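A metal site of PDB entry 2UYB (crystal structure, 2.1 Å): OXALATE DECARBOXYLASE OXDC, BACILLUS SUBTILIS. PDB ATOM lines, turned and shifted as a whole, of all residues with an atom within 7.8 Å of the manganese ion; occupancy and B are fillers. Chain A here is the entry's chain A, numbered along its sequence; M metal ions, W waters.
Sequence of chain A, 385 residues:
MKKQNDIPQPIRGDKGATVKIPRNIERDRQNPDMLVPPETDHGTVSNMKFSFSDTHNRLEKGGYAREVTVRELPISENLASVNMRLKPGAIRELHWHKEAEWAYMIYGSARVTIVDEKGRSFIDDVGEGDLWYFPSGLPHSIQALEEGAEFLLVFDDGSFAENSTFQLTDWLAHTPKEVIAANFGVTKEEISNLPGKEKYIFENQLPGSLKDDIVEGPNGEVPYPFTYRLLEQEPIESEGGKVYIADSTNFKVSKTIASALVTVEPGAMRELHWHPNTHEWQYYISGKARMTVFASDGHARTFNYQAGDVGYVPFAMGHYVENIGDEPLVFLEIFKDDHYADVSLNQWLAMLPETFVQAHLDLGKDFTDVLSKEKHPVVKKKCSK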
ATOM      1  N   VAL A 262     -16.093  -2.614 -19.779  1.00  0.00           N
ATOM      2  CA  VAL A 262     -14.980  -3.215 -19.075  1.00  0.00           C
ATOM      3  C   VAL A 262     -14.544  -4.512 -19.781  1.00  0.00           C
ATOM      4  O   VAL A 262     -15.363  -5.378 -20.079  1.00  0.00           O
ATOM      5  CB  VAL A 262     -15.375  -3.514 -17.639  1.00  0.00           C
ATOM      6  CG1 VAL A 262     -14.188  -4.074 -16.794  1.00  0.00           C
ATOM      7  CG2 VAL A 262     -16.030  -2.257 -16.997  1.00  0.00           C
ATOM      8  N   ARG A 270     -12.126  -7.294 -12.267  1.00  0.00           N
ATOM      9  CA  ARG A 270     -12.515  -5.932 -11.914  1.00  0.00           C
ATOM     10  C   ARG A 270     -12.380  -5.899 -10.376  1.00  0.00           C
ATOM     11  O   ARG A 270     -13.002  -6.708  -9.666  1.00  0.00           O
ATOM     12  CB  ARG A 270     -13.935  -5.646 -12.390  1.00  0.00           C
ATOM     13  CG  ARG A 270     -14.473  -4.275 -12.042  1.00  0.00           C
ATOM     14  CD  ARG A 270     -14.042  -3.200 -13.037  1.00  0.00           C
ATOM     15  NE  ARG A 270     -14.657  -1.957 -12.623  1.00  0.00           N
ATOM     16  CZ  ARG A 270     -14.214  -1.170 -11.650  1.00  0.00           C
ATOM     17  NH1 ARG A 270     -13.084  -1.453 -10.984  1.00  0.00           N
ATOM     18  NH2 ARG A 270     -14.897  -0.067 -11.326  1.00  0.00           N
ATOM     19  N   GLU A 271     -11.536  -5.011  -9.858  1.00  0.00           N
ATOM     20  CA  GLU A 271     -11.160  -5.062  -8.441  1.00  0.00           C
ATOM     21  C   GLU A 271     -12.365  -4.856  -7.481  1.00  0.00           C
ATOM     22  O   GLU A 271     -13.444  -4.422  -7.883  1.00  0.00           O
ATOM     23  CB  GLU A 271     -10.096  -4.022  -8.146  1.00  0.00           C
ATOM     24  CG  GLU A 271     -10.616  -2.597  -8.231  1.00  0.00           C
ATOM     25  CD  GLU A 271      -9.610  -1.549  -7.759  1.00  0.00           C
ATOM     26  OE1 GLU A 271      -8.566  -1.935  -7.176  1.00  0.00           O
ATOM     27  OE2 GLU A 271      -9.852  -0.355  -7.957  1.00  0.00           O
ATOM     28  N   HIS A 273     -14.571  -2.878  -5.285  1.00  0.00           N
ATOM     29  CA  HIS A 273     -14.929  -1.457  -5.299  1.00  0.00           C
ATOM     30  C   HIS A 273     -16.409  -1.291  -4.980  1.00  0.00           C
ATOM     31  O   HIS A 273     -17.147  -2.264  -4.848  1.00  0.00           O
ATOM     32  CB  HIS A 273     -14.634  -0.845  -6.681  1.00  0.00           C
ATOM     33  CG  HIS A 273     -15.530  -1.363  -7.757  1.00  0.00           C
ATOM     34  ND1 HIS A 273     -15.417  -2.641  -8.273  1.00  0.00           N
ATOM     35  CD2 HIS A 273     -16.545  -0.769  -8.432  1.00  0.00           C
ATOM     36  CE1 HIS A 273     -16.341  -2.815  -9.205  1.00  0.00           C
ATOM     37  NE2 HIS A 273     -17.027  -1.698  -9.319  1.00  0.00           N
ATOM     38  N   TRP A 274     -16.843  -0.029  -4.836  1.00  0.00           N
ATOM     39  CA  TRP A 274     -18.250   0.277  -4.874  1.00  0.00           C
ATOM     40  C   TRP A 274     -18.449   1.601  -5.571  1.00  0.00           C
ATOM     41  O   TRP A 274     -17.458   2.323  -5.937  1.00  0.00           O
ATOM     42  CB  TRP A 274     -18.910   0.260  -3.472  1.00  0.00           C
ATOM     43  CG  TRP A 274     -18.543   1.413  -2.561  1.00  0.00           C
ATOM     44  CD1 TRP A 274     -19.174   2.619  -2.439  1.00  0.00           C
ATOM     45  CD2 TRP A 274     -17.424   1.464  -1.678  1.00  0.00           C
ATOM     46  NE1 TRP A 274     -18.552   3.391  -1.506  1.00  0.00           N
ATOM     47  CE2 TRP A 274     -17.460   2.703  -1.026  1.00  0.00           C
ATOM     48  CE3 TRP A 274     -16.383   0.566  -1.374  1.00  0.00           C
ATOM     49  CZ2 TRP A 274     -16.496   3.094  -0.081  1.00  0.00           C
ATOM     50  CZ3 TRP A 274     -15.427   0.941  -0.415  1.00  0.00           C
ATOM     51  CH2 TRP A 274     -15.489   2.208   0.211  1.00  0.00           C
ATOM     52  N   HIS A 275     -19.720   1.921  -5.799  1.00  0.00           N
ATOM     53  CA  HIS A 275     -20.088   3.186  -6.439  1.00  0.00           C
ATOM     54  C   HIS A 275     -20.795   4.027  -5.421  1.00  0.00           C
ATOM     55  O   HIS A 275     -21.796   3.581  -4.836  1.00  0.00           O
ATOM     56  CB  HIS A 275     -20.917   2.910  -7.701  1.00  0.00           C
ATOM     57  CG  HIS A 275     -20.217   2.014  -8.663  1.00  0.00           C
ATOM     58  ND1 HIS A 275     -19.231   2.471  -9.531  1.00  0.00           N
ATOM     59  CD2 HIS A 275     -20.280   0.673  -8.835  1.00  0.00           C
ATOM     60  CE1 HIS A 275     -18.743   1.444 -10.210  1.00  0.00           C
ATOM     61  NE2 HIS A 275     -19.378   0.351  -9.816  1.00  0.00           N
ATOM     62  N   GLU A 280     -25.792   0.054  -9.883  1.00  0.00           N
ATOM     63  CA  GLU A 280     -25.184  -0.355 -11.145  1.00  0.00           C
ATOM     64  C   GLU A 280     -26.041  -1.427 -11.799  1.00  0.00           C
ATOM     65  O   GLU A 280     -26.376  -2.420 -11.175  1.00  0.00           O
ATOM     66  CB  GLU A 280     -23.809  -0.956 -10.869  1.00  0.00           C
ATOM     67  CG  GLU A 280     -23.115  -1.547 -12.125  1.00  0.00           C
ATOM     68  CD  GLU A 280     -21.749  -2.117 -11.801  1.00  0.00           C
ATOM     69  OE1 GLU A 280     -21.055  -1.489 -10.994  1.00  0.00           O
ATOM     70  OE2 GLU A 280     -21.357  -3.173 -12.333  1.00  0.00           O
ATOM     71  N   TRP A 281     -26.311  -1.258 -13.094  1.00  0.00           N
ATOM     72  CA  TRP A 281     -26.976  -2.267 -13.906  1.00  0.00           C
ATOM     73  C   TRP A 281     -25.878  -2.808 -14.856  1.00  0.00           C
ATOM     74  O   TRP A 281     -25.051  -2.041 -15.334  1.00  0.00           O
ATOM     75  CB  TRP A 281     -28.125  -1.565 -14.653  1.00  0.00           C
ATOM     76  CG  TRP A 281     -28.968  -2.454 -15.540  1.00  0.00           C
ATOM     77  CD1 TRP A 281     -30.189  -3.001 -15.240  1.00  0.00           C
ATOM     78  CD2 TRP A 281     -28.651  -2.867 -16.872  1.00  0.00           C
ATOM     79  NE1 TRP A 281     -30.650  -3.740 -16.303  1.00  0.00           N
ATOM     80  CE2 TRP A 281     -29.726  -3.689 -17.316  1.00  0.00           C
ATOM     81  CE3 TRP A 281     -27.568  -2.643 -17.728  1.00  0.00           C
ATOM     82  CZ2 TRP A 281     -29.736  -4.287 -18.591  1.00  0.00           C
ATOM     83  CZ3 TRP A 281     -27.572  -3.235 -19.006  1.00  0.00           C
ATOM     84  CH2 TRP A 281     -28.662  -4.029 -19.423  1.00  0.00           C
ATOM     85  N   GLN A 282     -25.840  -4.133 -15.070  1.00  0.00           N
ATOM     86  CA  GLN A 282     -24.751  -4.762 -15.856  1.00  0.00           C
ATOM     87  C   GLN A 282     -25.297  -5.532 -17.064  1.00  0.00           C
ATOM     88  O   GLN A 282     -26.347  -6.118 -16.963  1.00  0.00           O
ATOM     89  CB  GLN A 282     -23.986  -5.787 -14.991  1.00  0.00           C
ATOM     90  CG  GLN A 282     -23.406  -5.236 -13.714  1.00  0.00           C
ATOM     91  CD  GLN A 282     -22.729  -6.326 -12.886  1.00  0.00           C
ATOM     92  OE1 GLN A 282     -23.152  -7.504 -12.888  1.00  0.00           O
ATOM     93  NE2 GLN A 282     -21.672  -5.939 -12.191  1.00  0.00           N
ATOM     94  N   MET A 291     -19.517 -12.732  -9.435  1.00  0.00           N
ATOM     95  CA  MET A 291     -19.477 -11.539  -8.636  1.00  0.00           C
ATOM     96  C   MET A 291     -20.143 -11.827  -7.292  1.00  0.00           C
ATOM     97  O   MET A 291     -21.246 -12.369  -7.270  1.00  0.00           O
ATOM     98  CB  MET A 291     -20.249 -10.416  -9.342  1.00  0.00           C
ATOM     99  CG  MET A 291     -20.737  -9.325  -8.405  1.00  0.00           C
ATOM    100  SD  MET A 291     -21.334  -7.817  -9.209  1.00  0.00           S
ATOM    101  CE  MET A 291     -23.010  -8.347  -9.636  1.00  0.00           C
ATOM    102  N   VAL A 313     -26.158  -4.302  -9.119  1.00  0.00           N
ATOM    103  CA  VAL A 313     -25.541  -4.052  -7.813  1.00  0.00           C
ATOM    104  C   VAL A 313     -26.206  -2.832  -7.209  1.00  0.00           C
ATOM    105  O   VAL A 313     -25.926  -1.696  -7.645  1.00  0.00           O
ATOM    106  CB  VAL A 313     -24.009  -3.742  -7.893  1.00  0.00           C
ATOM    107  CG1 VAL A 313     -23.400  -3.782  -6.476  1.00  0.00           C
ATOM    108  CG2 VAL A 313     -23.284  -4.737  -8.767  1.00  0.00           C
ATOM    109  N   MET A 317     -23.278  -1.083  -2.630  1.00  0.00           N
ATOM    110  CA  MET A 317     -22.902  -2.440  -2.198  1.00  0.00           C
ATOM    111  C   MET A 317     -21.491  -2.831  -2.732  1.00  0.00           C
ATOM    112  O   MET A 317     -21.181  -2.557  -3.868  1.00  0.00           O
ATOM    113  CB  MET A 317     -23.963  -3.458  -2.627  1.00  0.00           C
ATOM    114  CG  MET A 317     -25.280  -3.272  -1.876  1.00  0.00           C
ATOM    115  SD  MET A 317     -26.336  -4.668  -2.133  1.00  0.00           S
ATOM    116  CE  MET A 317     -27.684  -4.284  -1.028  1.00  0.00           C
ATOM    117  N   GLY A 318     -20.668  -3.478  -1.910  1.00  0.00           N
ATOM    118  CA  GLY A 318     -19.284  -3.791  -2.300  1.00  0.00           C
ATOM    119  C   GLY A 318     -19.334  -4.915  -3.314  1.00  0.00           C
ATOM    120  O   GLY A 318     -20.198  -5.762  -3.232  1.00  0.00           O
ATOM    121  N   HIS A 319     -18.424  -4.946  -4.283  1.00  0.00           N
ATOM    122  CA  HIS A 319     -18.427  -6.012  -5.294  1.00  0.00           C
ATOM    123  C   HIS A 319     -17.107  -6.106  -6.030  1.00  0.00           C
ATOM    124  O   HIS A 319     -16.265  -5.192  -5.925  1.00  0.00           O
ATOM    125  CB  HIS A 319     -19.614  -5.878  -6.294  1.00  0.00           C
ATOM    126  CG  HIS A 319     -19.670  -4.579  -7.032  1.00  0.00           C
ATOM    127  ND1 HIS A 319     -20.019  -3.394  -6.419  1.00  0.00           N
ATOM    128  CD2 HIS A 319     -19.450  -4.283  -8.335  1.00  0.00           C
ATOM    129  CE1 HIS A 319     -19.994  -2.422  -7.313  1.00  0.00           C
ATOM    130  NE2 HIS A 319     -19.647  -2.934  -8.487  1.00  0.00           N
ATOM    131  N   TYR A 320     -16.944  -7.191  -6.778  1.00  0.00           N
ATOM    132  CA  TYR A 320     -15.808  -7.393  -7.714  1.00  0.00           C
ATOM    133  C   TYR A 320     -16.424  -8.167  -8.886  1.00  0.00           C
ATOM    134  O   TYR A 320     -17.506  -8.724  -8.757  1.00  0.00           O
ATOM    135  CB  TYR A 320     -14.687  -8.240  -7.050  1.00  0.00           C
ATOM    136  CG  TYR A 320     -15.158  -9.640  -6.692  1.00  0.00           C
ATOM    137  CD1 TYR A 320     -14.992 -10.703  -7.573  1.00  0.00           C
ATOM    138  CD2 TYR A 320     -15.803  -9.895  -5.480  1.00  0.00           C
ATOM    139  CE1 TYR A 320     -15.481 -11.998  -7.244  1.00  0.00           C
ATOM    140  CE2 TYR A 320     -16.248 -11.166  -5.140  1.00  0.00           C
ATOM    141  CZ  TYR A 320     -16.087 -12.220  -6.040  1.00  0.00           C
ATOM    142  OH  TYR A 320     -16.561 -13.486  -5.716  1.00  0.00           O
ATOM    143  N   VAL A 321     -15.765  -8.207 -10.040  1.00  0.00           N
ATOM    144  CA  VAL A 321     -16.221  -9.111 -11.100  1.00  0.00           C
ATOM    145  C   VAL A 321     -15.026  -9.889 -11.619  1.00  0.00           C
ATOM    146  O   VAL A 321     -14.140  -9.323 -12.275  1.00  0.00           O
ATOM    147  CB  VAL A 321     -16.925  -8.386 -12.286  1.00  0.00           C
ATOM    148  CG1 VAL A 321     -17.663  -9.433 -13.141  1.00  0.00           C
ATOM    149  CG2 VAL A 321     -17.893  -7.293 -11.790  1.00  0.00           C
ATOM    150  N   PHE A 331     -18.126  -6.665 -20.314  1.00  0.00           N
ATOM    151  CA  PHE A 331     -19.401  -6.310 -19.770  1.00  0.00           C
ATOM    152  C   PHE A 331     -19.540  -4.799 -19.647  1.00  0.00           C
ATOM    153  O   PHE A 331     -18.557  -4.077 -19.627  1.00  0.00           O
ATOM    154  CB  PHE A 331     -19.654  -7.017 -18.410  1.00  0.00           C
ATOM    155  CG  PHE A 331     -18.744  -6.586 -17.273  1.00  0.00           C
ATOM    156  CD1 PHE A 331     -19.160  -5.583 -16.378  1.00  0.00           C
ATOM    157  CD2 PHE A 331     -17.504  -7.208 -17.067  1.00  0.00           C
ATOM    158  CE1 PHE A 331     -18.335  -5.192 -15.312  1.00  0.00           C
ATOM    159  CE2 PHE A 331     -16.651  -6.818 -16.009  1.00  0.00           C
ATOM    160  CZ  PHE A 331     -17.078  -5.807 -15.117  1.00  0.00           C
ATOM    161  N   GLU A 333     -21.043  -1.576 -17.359  1.00  0.00           N
ATOM    162  CA  GLU A 333     -21.559  -1.066 -16.068  1.00  0.00           C
ATOM    163  C   GLU A 333     -22.359   0.180 -16.387  1.00  0.00           C
ATOM    164  O   GLU A 333     -21.812   1.107 -16.999  1.00  0.00           O
ATOM    165  CB  GLU A 333     -20.400  -0.698 -15.116  1.00  0.00           C
ATOM    166  CG  GLU A 333     -19.332  -1.773 -14.914  1.00  0.00           C
ATOM    167  CD  GLU A 333     -18.108  -1.285 -14.131  1.00  0.00           C
ATOM    168  OE1 GLU A 333     -17.696  -0.104 -14.269  1.00  0.00           O
ATOM    169  OE2 GLU A 333     -17.540  -2.092 -13.360  1.00  0.00           O
ATOM    170  N   ILE A 334     -23.647   0.198 -16.021  1.00  0.00           N
ATOM    171  CA  ILE A 334     -24.580   1.291 -16.375  1.00  0.00           C
ATOM    172  C   ILE A 334     -25.177   1.909 -15.082  1.00  0.00           C
ATOM    173  O   ILE A 334     -25.524   1.181 -14.141  1.00  0.00           O
ATOM    174  CB  ILE A 334     -25.744   0.771 -17.316  1.00  0.00           C
ATOM    175  CG1 ILE A 334     -25.171   0.087 -18.581  1.00  0.00           C
ATOM    176  CG2 ILE A 334     -26.768   1.875 -17.679  1.00  0.00           C
ATOM    177  CD1 ILE A 334     -24.394   0.974 -19.494  1.00  0.00           C
ATOM    178  N   PHE A 335     -25.296   3.236 -15.058  1.00  0.00           N
ATOM    179  CA  PHE A 335     -25.733   3.995 -13.886  1.00  0.00           C
ATOM    180  C   PHE A 335     -26.704   5.052 -14.331  1.00  0.00           C
ATOM    181  O   PHE A 335     -26.453   5.691 -15.345  1.00  0.00           O
ATOM    182  CB  PHE A 335     -24.536   4.657 -13.163  1.00  0.00           C
ATOM    183  CG  PHE A 335     -23.422   3.682 -12.813  1.00  0.00           C
ATOM    184  CD1 PHE A 335     -23.428   2.999 -11.583  1.00  0.00           C
ATOM    185  CD2 PHE A 335     -22.410   3.413 -13.737  1.00  0.00           C
ATOM    186  CE1 PHE A 335     -22.436   2.071 -11.287  1.00  0.00           C
ATOM    187  CE2 PHE A 335     -21.403   2.472 -13.467  1.00  0.00           C
ATOM    188  CZ  PHE A 335     -21.407   1.806 -12.260  1.00  0.00           C
ATOM    189  N   TYR A 340     -19.942   8.858 -13.857  1.00  0.00           N
ATOM    190  CA  TYR A 340     -19.383   7.636 -13.330  1.00  0.00           C
ATOM    191  C   TYR A 340     -18.541   7.977 -12.088  1.00  0.00           C
ATOM    192  O   TYR A 340     -17.819   8.969 -12.119  1.00  0.00           O
ATOM    193  CB  TYR A 340     -18.480   7.000 -14.383  1.00  0.00           C
ATOM    194  CG  TYR A 340     -17.947   5.649 -13.960  1.00  0.00           C
ATOM    195  CD1 TYR A 340     -18.549   4.476 -14.404  1.00  0.00           C
ATOM    196  CD2 TYR A 340     -16.822   5.543 -13.147  1.00  0.00           C
ATOM    197  CE1 TYR A 340     -18.069   3.220 -14.012  1.00  0.00           C
ATOM    198  CE2 TYR A 340     -16.338   4.324 -12.764  1.00  0.00           C
ATOM    199  CZ  TYR A 340     -16.962   3.160 -13.203  1.00  0.00           C
ATOM    200  OH  TYR A 340     -16.466   1.954 -12.826  1.00  0.00           O
ATOM    201  N   ALA A 341     -18.624   7.171 -11.025  1.00  0.00           N
ATOM    202  CA  ALA A 341     -17.709   7.267  -9.905  1.00  0.00           C
ATOM    203  C   ALA A 341     -17.584   5.903  -9.226  1.00  0.00           C
ATOM    204  O   ALA A 341     -18.554   5.148  -9.164  1.00  0.00           O
ATOM    205  CB  ALA A 341     -18.183   8.332  -8.872  1.00  0.00           C
ATOM    206  N   ASP A 342     -16.365   5.583  -8.765  1.00  0.00           N
ATOM    207  CA  ASP A 342     -16.128   4.406  -7.957  1.00  0.00           C
ATOM    208  C   ASP A 342     -15.173   4.711  -6.813  1.00  0.00           C
ATOM    209  O   ASP A 342     -14.427   5.705  -6.823  1.00  0.00           O
ATOM    210  CB  ASP A 342     -15.686   3.156  -8.769  1.00  0.00           C
ATOM    211  CG  ASP A 342     -14.292   3.315  -9.472  1.00  0.00           C
ATOM    212  OD1 ASP A 342     -13.742   4.423  -9.607  1.00  0.00           O
ATOM    213  OD2 ASP A 342     -13.761   2.302  -9.944  1.00  0.00           O
HETATM  214 MN    MN M   1     -19.091  -1.682 -10.274  1.00  0.00          MN
HETATM  215  O   HOH W   1     -18.712  -3.409 -11.687  1.00  0.00           O
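The side-chain carboxylate (OE1) of Glu 280 binds the manganese ion, at 2.1 Å. NE2 of His 275 binds the manganese ion. The manganese ion is bound by NE2 of His 319. Water W1 binds the manganese ion (2.3 Å). The manganese ion is bound by NE2 of His 273. The manganese ion has five donor atoms within binding distance.
Water W1 bridges the side-chain carboxylate (OE2) of Glu 333 (2.4 Å) and the side-chain carboxylate (OE2) of Glu 280 (2.7 Å).
OE2 of Glu 333 touches the manganese ion, at 3.5 Å. Five residues have an atom within 4 Å of the manganese ion: His 273, His 275, Glu 280, His 319 and Glu 333.
The backbone carbonyl oxygen (O) of Glu 280 sits at hydrogen-bond distance from the backbone NH (N) of Val 313 (2.8 Å). The backbone carbonyl oxygen (O) of Met 317 sits at hydrogen-bond distance from a ring nitrogen (ND1) of His 319. O of Glu 271 lies within hydrogen-bond range of ND1 of His 273, 2.7 Å away. The side-chain carboxylate (OE2) of Glu 333 lies within salt-bridge range of the guanidinium group (NE) of Arg 270, 3.0 Å away. ND1 of His 275 is in hydrogen-bond range of O of Ala 341 (2.8 Å). The side-chain hydroxyl (OH) of Tyr 340 lies within hydrogen-bond range of the side-chain carboxylate (OE1) of Glu 333 (2.8 Å). NE2 of His 273 lies close to NH2 of Arg 270, 3.4 Å away. OE2 of Glu 280 lies within hydrogen-bond range of NE2 of Gln 282 (2.8 Å).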
